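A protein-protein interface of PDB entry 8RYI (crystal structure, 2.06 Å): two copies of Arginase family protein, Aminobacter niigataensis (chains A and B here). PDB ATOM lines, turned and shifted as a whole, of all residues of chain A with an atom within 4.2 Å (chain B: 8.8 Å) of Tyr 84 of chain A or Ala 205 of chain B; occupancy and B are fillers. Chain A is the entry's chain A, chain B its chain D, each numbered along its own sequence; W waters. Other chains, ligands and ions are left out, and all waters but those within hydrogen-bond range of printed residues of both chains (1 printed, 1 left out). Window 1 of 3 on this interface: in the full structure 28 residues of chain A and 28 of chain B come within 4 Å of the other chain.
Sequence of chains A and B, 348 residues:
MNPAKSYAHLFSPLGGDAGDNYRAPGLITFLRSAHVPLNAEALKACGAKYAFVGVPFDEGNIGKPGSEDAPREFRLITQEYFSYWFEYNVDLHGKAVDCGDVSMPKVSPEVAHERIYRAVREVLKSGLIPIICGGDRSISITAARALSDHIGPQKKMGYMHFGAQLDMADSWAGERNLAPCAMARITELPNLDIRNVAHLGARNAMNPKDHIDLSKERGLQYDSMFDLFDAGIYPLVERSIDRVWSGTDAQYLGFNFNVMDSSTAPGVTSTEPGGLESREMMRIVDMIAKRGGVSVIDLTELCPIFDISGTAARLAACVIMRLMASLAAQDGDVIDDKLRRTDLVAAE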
ATOM      1  N   LEU A  10      24.318  13.020  32.660  1.00  0.00           N
ATOM      2  CA  LEU A  10      24.006  11.595  32.644  1.00  0.00           C
ATOM      3  C   LEU A  10      22.706  11.299  31.918  1.00  0.00           C
ATOM      4  O   LEU A  10      22.470  10.146  31.534  1.00  0.00           O
ATOM      5  CB  LEU A  10      23.892  11.059  34.074  1.00  0.00           C
ATOM      6  CG  LEU A  10      25.094  11.127  35.011  1.00  0.00           C
ATOM      7  CD1 LEU A  10      24.697  10.576  36.371  1.00  0.00           C
ATOM      8  CD2 LEU A  10      26.258  10.356  34.443  1.00  0.00           C
ATOM      9  N   PHE A  82      28.249  10.859  24.371  1.00  0.00           N
ATOM     10  CA  PHE A  82      27.886  11.090  25.755  1.00  0.00           C
ATOM     11  C   PHE A  82      28.948  10.484  26.661  1.00  0.00           C
ATOM     12  O   PHE A  82      29.718   9.605  26.257  1.00  0.00           O
ATOM     13  CB  PHE A  82      26.527  10.477  26.075  1.00  0.00           C
ATOM     14  CG  PHE A  82      25.371  11.318  25.653  1.00  0.00           C
ATOM     15  CD1 PHE A  82      25.016  11.417  24.319  1.00  0.00           C
ATOM     16  CD2 PHE A  82      24.653  12.035  26.599  1.00  0.00           C
ATOM     17  CE1 PHE A  82      23.954  12.196  23.929  1.00  0.00           C
ATOM     18  CE2 PHE A  82      23.588  12.828  26.224  1.00  0.00           C
ATOM     19  CZ  PHE A  82      23.239  12.905  24.872  1.00  0.00           C
ATOM     20  N   SER A  83      29.000  10.976  27.897  1.00  0.00           N
ATOM     21  CA  SER A  83      29.995  10.469  28.826  1.00  0.00           C
ATOM     22  C   SER A  83      29.544   9.238  29.595  1.00  0.00           C
ATOM     23  O   SER A  83      30.397   8.522  30.124  1.00  0.00           O
ATOM     24  CB  SER A  83      30.389  11.563  29.820  1.00  0.00           C
ATOM     25  OG  SER A  83      29.260  12.026  30.531  1.00  0.00           O
ATOM     26  N   TYR A  84      28.247   8.933  29.625  1.00  0.00           N
ATOM     27  CA  TYR A  84      27.750   7.829  30.436  1.00  0.00           C
ATOM     28  C   TYR A  84      27.669   6.564  29.589  1.00  0.00           C
ATOM     29  O   TYR A  84      27.115   6.585  28.482  1.00  0.00           O
ATOM     30  CB  TYR A  84      26.378   8.157  31.028  1.00  0.00           C
ATOM     31  CG  TYR A  84      25.761   6.998  31.784  1.00  0.00           C
ATOM     32  CD1 TYR A  84      26.211   6.665  33.055  1.00  0.00           C
ATOM     33  CD2 TYR A  84      24.741   6.234  31.230  1.00  0.00           C
ATOM     34  CE1 TYR A  84      25.675   5.613  33.748  1.00  0.00           C
ATOM     35  CE2 TYR A  84      24.187   5.180  31.932  1.00  0.00           C
ATOM     36  CZ  TYR A  84      24.664   4.869  33.186  1.00  0.00           C
ATOM     37  OH  TYR A  84      24.131   3.815  33.896  1.00  0.00           O
ATOM     38  N   TRP A  85      28.201   5.457  30.124  1.00  0.00           N
ATOM     39  CA  TRP A  85      28.236   4.168  29.426  1.00  0.00           C
ATOM     40  C   TRP A  85      27.344   3.179  30.173  1.00  0.00           C
ATOM     41  O   TRP A  85      27.727   2.666  31.228  1.00  0.00           O
ATOM     42  CB  TRP A  85      29.669   3.663  29.331  1.00  0.00           C
ATOM     43  CG  TRP A  85      30.460   4.437  28.368  1.00  0.00           C
ATOM     44  CD1 TRP A  85      30.958   5.693  28.546  1.00  0.00           C
ATOM     45  CD2 TRP A  85      30.824   4.044  27.040  1.00  0.00           C
ATOM     46  NE1 TRP A  85      31.623   6.097  27.425  1.00  0.00           N
ATOM     47  CE2 TRP A  85      31.555   5.104  26.482  1.00  0.00           C
ATOM     48  CE3 TRP A  85      30.598   2.899  26.270  1.00  0.00           C
ATOM     49  CZ2 TRP A  85      32.068   5.055  25.193  1.00  0.00           C
ATOM     50  CZ3 TRP A  85      31.103   2.852  24.995  1.00  0.00           C
ATOM     51  CH2 TRP A  85      31.837   3.918  24.468  1.00  0.00           C
ATOM     52  N   PHE A  86      26.151   2.910  29.631  1.00  0.00           N
ATOM     53  CA  PHE A  86      25.227   2.032  30.347  1.00  0.00           C
ATOM     54  C   PHE A  86      25.782   0.621  30.477  1.00  0.00           C
ATOM     55  O   PHE A  86      25.449  -0.083  31.431  1.00  0.00           O
ATOM     56  CB  PHE A  86      23.858   2.012  29.656  1.00  0.00           C
ATOM     57  CG  PHE A  86      23.775   1.070  28.462  1.00  0.00           C
ATOM     58  CD1 PHE A  86      24.325   1.432  27.241  1.00  0.00           C
ATOM     59  CD2 PHE A  86      23.118  -0.144  28.568  1.00  0.00           C
ATOM     60  CE1 PHE A  86      24.262   0.583  26.139  1.00  0.00           C
ATOM     61  CE2 PHE A  86      23.028  -1.001  27.478  1.00  0.00           C
ATOM     62  CZ  PHE A  86      23.604  -0.640  26.256  1.00  0.00           C
ATOM     63  N   ASN A  89      27.815   1.225  33.670  1.00  0.00           N
ATOM     64  CA  ASN A  89      27.299   2.115  34.717  1.00  0.00           C
ATOM     65  C   ASN A  89      28.376   3.109  35.156  1.00  0.00           C
ATOM     66  O   ASN A  89      28.543   3.395  36.344  1.00  0.00           O
ATOM     67  CB  ASN A  89      26.750   1.334  35.915  1.00  0.00           C
ATOM     68  CG  ASN A  89      25.948   2.221  36.878  1.00  0.00           C
ATOM     69  OD1 ASN A  89      25.325   3.202  36.458  1.00  0.00           O
ATOM     70  ND2 ASN A  89      25.964   1.883  38.173  1.00  0.00           N
ATOM     71  N   VAL A  90      29.108   3.650  34.185  1.00  0.00           N
ATOM     72  CA  VAL A  90      30.259   4.509  34.442  1.00  0.00           C
ATOM     73  C   VAL A  90      30.075   5.845  33.726  1.00  0.00           C
ATOM     74  O   VAL A  90      29.583   5.896  32.592  1.00  0.00           O
ATOM     75  CB  VAL A  90      31.560   3.808  33.999  1.00  0.00           C
ATOM     76  CG1 VAL A  90      32.697   4.796  33.865  1.00  0.00           C
ATOM     77  CG2 VAL A  90      31.899   2.695  34.987  1.00  0.00           C
ATOM     78  N   ILE A 335      28.400   4.824  38.994  1.00  0.00           N
ATOM     79  CA  ILE A 335      27.538   5.862  39.525  1.00  0.00           C
ATOM     80  C   ILE A 335      26.409   5.204  40.308  1.00  0.00           C
ATOM     81  O   ILE A 335      26.057   4.039  40.091  1.00  0.00           O
ATOM     82  CB  ILE A 335      26.970   6.782  38.433  1.00  0.00           C
ATOM     83  CG1 ILE A 335      25.939   6.033  37.626  1.00  0.00           C
ATOM     84  CG2 ILE A 335      28.063   7.250  37.476  1.00  0.00           C
ATOM     85  CD1 ILE A 335      24.742   6.867  37.445  1.00  0.00           C
ATOM     86  N   ALA B 164      21.100   0.537  17.699  1.00  0.00           N
ATOM     87  CA  ALA B 164      22.104   0.673  18.746  1.00  0.00           C
ATOM     88  C   ALA B 164      21.615   1.489  19.936  1.00  0.00           C
ATOM     89  O   ALA B 164      22.260   1.462  20.989  1.00  0.00           O
ATOM     90  CB  ALA B 164      23.381   1.305  18.184  1.00  0.00           C
ATOM     91  N   GLN B 165      20.510   2.216  19.782  1.00  0.00           N
ATOM     92  CA  GLN B 165      20.002   3.137  20.788  1.00  0.00           C
ATOM     93  C   GLN B 165      18.623   2.704  21.253  1.00  0.00           C
ATOM     94  O   GLN B 165      17.761   2.360  20.437  1.00  0.00           O
ATOM     95  CB  GLN B 165      19.932   4.547  20.232  1.00  0.00           C
ATOM     96  CG  GLN B 165      21.286   5.108  19.882  1.00  0.00           C
ATOM     97  CD  GLN B 165      21.194   6.101  18.767  1.00  0.00           C
ATOM     98  OE1 GLN B 165      21.148   5.721  17.599  1.00  0.00           O
ATOM     99  NE2 GLN B 165      21.142   7.382  19.109  1.00  0.00           N
ATOM    100  N   TRP B 172      12.944  14.969  25.762  1.00  0.00           N
ATOM    101  CA  TRP B 172      14.260  15.372  25.284  1.00  0.00           C
ATOM    102  C   TRP B 172      14.176  16.834  24.876  1.00  0.00           C
ATOM    103  O   TRP B 172      13.345  17.193  24.039  1.00  0.00           O
ATOM    104  CB  TRP B 172      14.699  14.492  24.105  1.00  0.00           C
ATOM    105  CG  TRP B 172      16.092  14.733  23.604  1.00  0.00           C
ATOM    106  CD1 TRP B 172      16.525  15.777  22.840  1.00  0.00           C
ATOM    107  CD2 TRP B 172      17.233  13.900  23.829  1.00  0.00           C
ATOM    108  NE1 TRP B 172      17.866  15.645  22.576  1.00  0.00           N
ATOM    109  CE2 TRP B 172      18.325  14.502  23.173  1.00  0.00           C
ATOM    110  CE3 TRP B 172      17.438  12.703  24.525  1.00  0.00           C
ATOM    111  CZ2 TRP B 172      19.601  13.947  23.186  1.00  0.00           C
ATOM    112  CZ3 TRP B 172      18.709  12.154  24.541  1.00  0.00           C
ATOM    113  CH2 TRP B 172      19.775  12.776  23.874  1.00  0.00           C
ATOM    114  N   ALA B 202      21.315  -2.709  21.428  1.00  0.00           N
ATOM    115  CA  ALA B 202      21.776  -1.536  22.166  1.00  0.00           C
ATOM    116  C   ALA B 202      23.205  -1.711  22.663  1.00  0.00           C
ATOM    117  O   ALA B 202      23.568  -2.758  23.206  1.00  0.00           O
ATOM    118  CB  ALA B 202      20.849  -1.250  23.349  1.00  0.00           C
ATOM    119  N   ARG B 203      24.009  -0.660  22.509  1.00  0.00           N
ATOM    120  CA  ARG B 203      25.418  -0.701  22.885  1.00  0.00           C
ATOM    121  C   ARG B 203      25.969   0.721  22.901  1.00  0.00           C
ATOM    122  O   ARG B 203      25.362   1.647  22.357  1.00  0.00           O
ATOM    123  CB  ARG B 203      26.199  -1.583  21.913  1.00  0.00           C
ATOM    124  CG  ARG B 203      26.185  -1.059  20.480  1.00  0.00           C
ATOM    125  CD  ARG B 203      26.943  -2.010  19.561  1.00  0.00           C
ATOM    126  NE  ARG B 203      27.106  -1.508  18.202  1.00  0.00           N
ATOM    127  CZ  ARG B 203      26.159  -1.546  17.269  1.00  0.00           C
ATOM    128  NH1 ARG B 203      24.927  -1.951  17.545  1.00  0.00           N
ATOM    129  NH2 ARG B 203      26.462  -1.209  16.018  1.00  0.00           N
ATOM    130  N   ASN B 204      27.136   0.879  23.525  1.00  0.00           N
ATOM    131  CA  ASN B 204      27.892   2.132  23.528  1.00  0.00           C
ATOM    132  C   ASN B 204      27.162   3.290  24.197  1.00  0.00           C
ATOM    133  O   ASN B 204      26.174   3.088  24.907  1.00  0.00           O
ATOM    134  CB  ASN B 204      28.306   2.503  22.102  1.00  0.00           C
ATOM    135  CG  ASN B 204      29.155   1.427  21.463  1.00  0.00           C
ATOM    136  OD1 ASN B 204      29.814   0.644  22.164  1.00  0.00           O
ATOM    137  ND2 ASN B 204      29.127   1.355  20.140  1.00  0.00           N
ATOM    138  N   ALA B 205      27.683   4.501  24.047  1.00  0.00           N
ATOM    139  CA  ALA B 205      27.373   5.561  24.996  1.00  0.00           C
ATOM    140  C   ALA B 205      26.228   6.471  24.576  1.00  0.00           C
ATOM    141  O   ALA B 205      25.984   7.464  25.256  1.00  0.00           O
ATOM    142  CB  ALA B 205      28.618   6.409  25.251  1.00  0.00           C
ATOM    143  N   MET B 206      25.499   6.164  23.515  1.00  0.00           N
ATOM    144  CA  MET B 206      24.371   7.030  23.165  1.00  0.00           C
ATOM    145  C   MET B 206      23.075   6.538  23.815  1.00  0.00           C
ATOM    146  O   MET B 206      22.016   6.454  23.198  1.00  0.00           O
ATOM    147  CB  MET B 206      24.246   7.139  21.647  1.00  0.00           C
ATOM    148  CG  MET B 206      25.567   7.535  20.948  1.00  0.00           C
ATOM    149  SD  MET B 206      26.459   8.966  21.646  1.00  0.00           S
ATOM    150  CE  MET B 206      25.511  10.338  20.985  1.00  0.00           C
ATOM    151  N   ASN B 207      23.163   6.224  25.105  1.00  0.00           N
ATOM    152  CA  ASN B 207      22.048   5.655  25.857  1.00  0.00           C
ATOM    153  C   ASN B 207      22.125   6.214  27.273  1.00  0.00           C
ATOM    154  O   ASN B 207      22.729   5.605  28.166  1.00  0.00           O
ATOM    155  CB  ASN B 207      22.095   4.127  25.865  1.00  0.00           C
ATOM    156  CG  ASN B 207      21.805   3.516  24.500  1.00  0.00           C
ATOM    157  OD1 ASN B 207      20.656   3.487  24.038  1.00  0.00           O
ATOM    158  ND2 ASN B 207      22.845   2.991  23.861  1.00  0.00           N
ATOM    159  N   PRO B 208      21.546   7.389  27.508  1.00  0.00           N
ATOM    160  CA  PRO B 208      21.661   8.018  28.829  1.00  0.00           C
ATOM    161  C   PRO B 208      20.923   7.210  29.889  1.00  0.00           C
ATOM    162  O   PRO B 208      20.108   6.339  29.585  1.00  0.00           O
ATOM    163  CB  PRO B 208      21.013   9.393  28.633  1.00  0.00           C
ATOM    164  CG  PRO B 208      20.879   9.571  27.133  1.00  0.00           C
ATOM    165  CD  PRO B 208      20.730   8.188  26.580  1.00  0.00           C
ATOM    166  N   LYS B 209      21.224   7.513  31.155  1.00  0.00           N
ATOM    167  CA  LYS B 209      20.766   6.652  32.247  1.00  0.00           C
ATOM    168  C   LYS B 209      19.245   6.600  32.342  1.00  0.00           C
ATOM    169  O   LYS B 209      18.678   5.538  32.625  1.00  0.00           O
ATOM    170  CB  LYS B 209      21.344   7.110  33.581  1.00  0.00           C
ATOM    171  CG  LYS B 209      20.978   6.161  34.719  1.00  0.00           C
ATOM    172  CD  LYS B 209      21.678   6.504  36.015  1.00  0.00           C
ATOM    173  CE  LYS B 209      21.489   5.413  37.064  1.00  0.00           C
ATOM    174  NZ  LYS B 209      20.059   5.197  37.399  1.00  0.00           N
ATOM    175  N   ASP B 210      18.563   7.726  32.100  1.00  0.00           N
ATOM    176  CA  ASP B 210      17.105   7.699  32.170  1.00  0.00           C
ATOM    177  C   ASP B 210      16.493   6.806  31.088  1.00  0.00           C
ATOM    178  O   ASP B 210      15.336   6.395  31.228  1.00  0.00           O
ATOM    179  CB  ASP B 210      16.512   9.117  32.102  1.00  0.00           C
ATOM    180  CG  ASP B 210      16.893   9.866  30.836  1.00  0.00           C
ATOM    181  OD1 ASP B 210      18.090  10.143  30.632  1.00  0.00           O
ATOM    182  OD2 ASP B 210      15.987  10.173  30.033  1.00  0.00           O
ATOM    183  N   HIS B 211      17.217   6.508  30.005  1.00  0.00           N
ATOM    184  CA  HIS B 211      16.686   5.517  29.066  1.00  0.00           C
ATOM    185  C   HIS B 211      16.713   4.118  29.677  1.00  0.00           C
ATOM    186  O   HIS B 211      15.796   3.319  29.453  1.00  0.00           O
ATOM    187  CB  HIS B 211      17.453   5.529  27.744  1.00  0.00           C
ATOM    188  CG  HIS B 211      17.353   6.820  26.995  1.00  0.00           C
ATOM    189  ND1 HIS B 211      17.506   6.899  25.624  1.00  0.00           N
ATOM    190  CD2 HIS B 211      17.148   8.089  27.426  1.00  0.00           C
ATOM    191  CE1 HIS B 211      17.389   8.159  25.245  1.00  0.00           C
ATOM    192  NE2 HIS B 211      17.177   8.901  26.320  1.00  0.00           N
ATOM    193  N   ILE B 212      17.760   3.802  30.438  1.00  0.00           N
ATOM    194  CA  ILE B 212      17.830   2.522  31.140  1.00  0.00           C
ATOM    195  C   ILE B 212      16.914   2.516  32.358  1.00  0.00           C
ATOM    196  O   ILE B 212      16.278   1.498  32.665  1.00  0.00           O
ATOM    197  CB  ILE B 212      19.286   2.168  31.505  1.00  0.00           C
ATOM    198  CG1 ILE B 212      20.082   1.828  30.235  1.00  0.00           C
ATOM    199  CG2 ILE B 212      19.336   1.010  32.492  1.00  0.00           C
ATOM    200  CD1 ILE B 212      20.499   3.012  29.393  1.00  0.00           C
ATOM    201  N   ASP B 213      16.865   3.620  33.104  1.00  0.00           N
ATOM    202  CA  ASP B 213      15.955   3.684  34.239  1.00  0.00           C
ATOM    203  C   ASP B 213      14.513   3.475  33.787  1.00  0.00           C
ATOM    204  O   ASP B 213      13.772   2.682  34.378  1.00  0.00           O
ATOM    205  CB  ASP B 213      16.115   5.023  34.962  1.00  0.00           C
ATOM    206  CG  ASP B 213      17.511   5.207  35.555  1.00  0.00           C
ATOM    207  OD1 ASP B 213      18.225   4.196  35.736  1.00  0.00           O
ATOM    208  OD2 ASP B 213      17.888   6.364  35.860  1.00  0.00           O
ATOM    209  N   LYS B 216      13.879  -0.131  32.739  1.00  0.00           N
ATOM    210  CA  LYS B 216      13.707  -1.015  33.888  1.00  0.00           C
ATOM    211  C   LYS B 216      12.347  -0.811  34.541  1.00  0.00           C
ATOM    212  O   LYS B 216      11.708  -1.780  34.961  1.00  0.00           O
ATOM    213  CB  LYS B 216      14.820  -0.799  34.912  1.00  0.00           C
ATOM    214  CG  LYS B 216      15.969  -1.794  34.806  1.00  0.00           C
ATOM    215  CD  LYS B 216      17.210  -1.279  35.529  1.00  0.00           C
ATOM    216  CE  LYS B 216      18.451  -2.094  35.166  1.00  0.00           C
ATOM    217  NZ  LYS B 216      19.713  -1.360  35.518  1.00  0.00           N
ATOM    218  N   TYR B 222      15.056  -5.568  26.747  1.00  0.00           N
ATOM    219  CA  TYR B 222      15.811  -5.357  25.523  1.00  0.00           C
ATOM    220  C   TYR B 222      17.004  -6.304  25.499  1.00  0.00           C
ATOM    221  O   TYR B 222      17.560  -6.664  26.539  1.00  0.00           O
ATOM    222  CB  TYR B 222      16.265  -3.897  25.406  1.00  0.00           C
ATOM    223  CG  TYR B 222      17.130  -3.433  26.557  1.00  0.00           C
ATOM    224  CD1 TYR B 222      18.501  -3.656  26.551  1.00  0.00           C
ATOM    225  CD2 TYR B 222      16.578  -2.773  27.658  1.00  0.00           C
ATOM    226  CE1 TYR B 222      19.303  -3.246  27.605  1.00  0.00           C
ATOM    227  CE2 TYR B 222      17.386  -2.353  28.730  1.00  0.00           C
ATOM    228  CZ  TYR B 222      18.749  -2.592  28.678  1.00  0.00           C
ATOM    229  OH  TYR B 222      19.579  -2.199  29.702  1.00  0.00           O
ATOM    230  N   SER B 270      23.893   7.591  12.774  1.00  0.00           N
ATOM    231  CA  SER B 270      24.798   7.549  13.920  1.00  0.00           C
ATOM    232  C   SER B 270      25.436   6.164  13.981  1.00  0.00           C
ATOM    233  O   SER B 270      24.938   5.272  14.671  1.00  0.00           O
ATOM    234  CB  SER B 270      24.072   7.902  15.205  1.00  0.00           C
ATOM    235  OG  SER B 270      25.020   8.052  16.245  1.00  0.00           O
ATOM    236  N   GLU B 272      27.957   3.004  14.717  1.00  0.00           N
ATOM    237  CA  GLU B 272      28.471   2.480  15.991  1.00  0.00           C
ATOM    238  C   GLU B 272      29.290   1.207  15.800  1.00  0.00           C
ATOM    239  O   GLU B 272      28.790   0.233  15.217  1.00  0.00           O
ATOM    240  CB  GLU B 272      27.323   2.205  16.972  1.00  0.00           C
ATOM    241  CG  GLU B 272      26.638   3.440  17.554  1.00  0.00           C
ATOM    242  CD  GLU B 272      27.488   4.165  18.587  1.00  0.00           C
ATOM    243  OE1 GLU B 272      28.682   3.823  18.765  1.00  0.00           O
ATOM    244  OE2 GLU B 272      26.940   5.060  19.269  1.00  0.00           O
ATOM    245  N   PRO B 273      30.520   1.161  16.303  1.00  0.00           N
ATOM    246  CA  PRO B 273      31.301  -0.080  16.226  1.00  0.00           C
ATOM    247  C   PRO B 273      30.698  -1.168  17.115  1.00  0.00           C
ATOM    248  O   PRO B 273      29.915  -0.901  18.027  1.00  0.00           O
ATOM    249  CB  PRO B 273      32.691   0.332  16.725  1.00  0.00           C
ATOM    250  CG  PRO B 273      32.665   1.841  16.827  1.00  0.00           C
ATOM    251  CD  PRO B 273      31.237   2.241  17.000  1.00  0.00           C
HETATM  252  O   HOH W   1      27.515   1.536  26.977  1.00  0.00           O
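OH of Tyr 84 of chain A sits at hydrogen-bond distance from OD1 of Asn 89 of chain A (2.9 Å). The backbone carbonyl oxygen (O) of Ala 164 of chain B is in hydrogen-bond range of the side-chain amide nitrogen (ND2) of Asn 207 of chain B (3.3 Å). O of Arg 203 of chain B is in hydrogen-bond range of ND2 of Asn 207 of chain B (3.2 Å). The backbone carbonyl oxygen of Glu 272 of chain B lies within hydrogen-bond range of the guanidinium group of Arg 203 of chain B (2.9 Å). O of Pro 273 of chain B sits at hydrogen-bond distance from NE of Arg 203 of chain B (2.9 Å). The side-chain amide nitrogen of Asn 204 of chain B lies within hydrogen-bond range of the backbone carbonyl oxygen of Pro 273 of chain B (3.2 Å).
The backbone NH of Lys 209 of chain B lies within hydrogen-bond range of the backbone carbonyl oxygen of Leu 10 of chain A (2.9 Å). SD of Met 206 of chain B sits at hydrogen-bond distance from N of Phe 82 of chain A.
Hydrophobic or aromatic side chains of chain B that line the printed part of chain A: Trp 172, Ala 205, Met 206, Pro 208 and Ile 212. Of the 9 printed residues of chain A, 6 touch a printed residue of chain B. Hydrophobic or aromatic side chains of chain A within 4 Å of the printed part of chain B: Phe 82, Tyr 84, Trp 85, Phe 86 and Ile 335. Along chain A the printed residues that touch a printed residue of chain B span positions 10 to 335. Among the printed residues, 16 pairs touch across the chains. Among the printed residues, no Asp or Glu carboxylate lies within 4 Å of a Lys or Arg side-chain nitrogen of the other chain.
Among the printed residues, pairs that only touch across the chains: Phe 82 of chain A with Ala 205 of chain B (3.2 Å), Leu 10 of chain A with Pro 208 of chain B (3.3 Å), Phe 86 of chain A with Asn 204 of chain B (3.4 Å), Ile 335 of chain A with Lys 209 of chain B (3.4 Å), Trp 85 of chain A with Ala 205 of chain B (3.4 Å), Phe 86 of chain A with Ile 212 of chain B (3.5 Å), Tyr 84 of chain A with Ala 205 of chain B (3.5 Å), Trp 85 of chain A with Asn 204 of chain B (3.6 Å), Phe 86 of chain A with Asn 207 of chain B (3.6 Å), Phe 82 of chain A with Trp 172 of chain B (3.6 Å), Phe 86 of chain A with Arg 203 of chain B (3.7 Å), Phe 86 of chain A with Ala 202 of chain B (3.7 Å), Tyr 84 of chain A with Asn 207 of chain B (3.7 Å) and Tyr 84 of chain A with Lys 209 of chain B (3.7 Å).
Water W1 lies within hydrogen-bond range of O of Asn 204 of chain B (2.9 Å) and N of Phe 86 of chain A (3.3 Å).
Of chain B, only Ala 205 (3.5 Å), Asn 207 (3.7 Å) and Lys 209 (3.7 Å) come within 4 Å of Tyr 84 of chain A. Ala 205 of chain B touches just these residues of chain A: Phe 82, Tyr 84 and Trp 85. Trp 85 of chain A touches just these residues of chain B: Asn 204 and Ala 205. Printed residues of chain A within 4 Å of Arg 203 of chain B: Phe 86. Of the printed residues of chain A, Trp 172 of chain B touches Phe 82. Of the printed residues of chain A, Met 206 of chain B touches Phe 82 (3.5 Å). Printed residues of chain A within 4 Å of Asn 207 of chain B: Tyr 84 and Phe 86. Lys 216 of chain B touches none of the printed residues of chain A. Asp 210 of chain B touches none of the printed residues of chain A. The nearest residue of chain B that does not touch Tyr 84 of chain A is Pro 208 of chain B (4.2 Å).
No position is printed for both chains. Of the 16 pairs that touch across the chains among the printed residues, none has its exchanged pair printed and touching as well.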
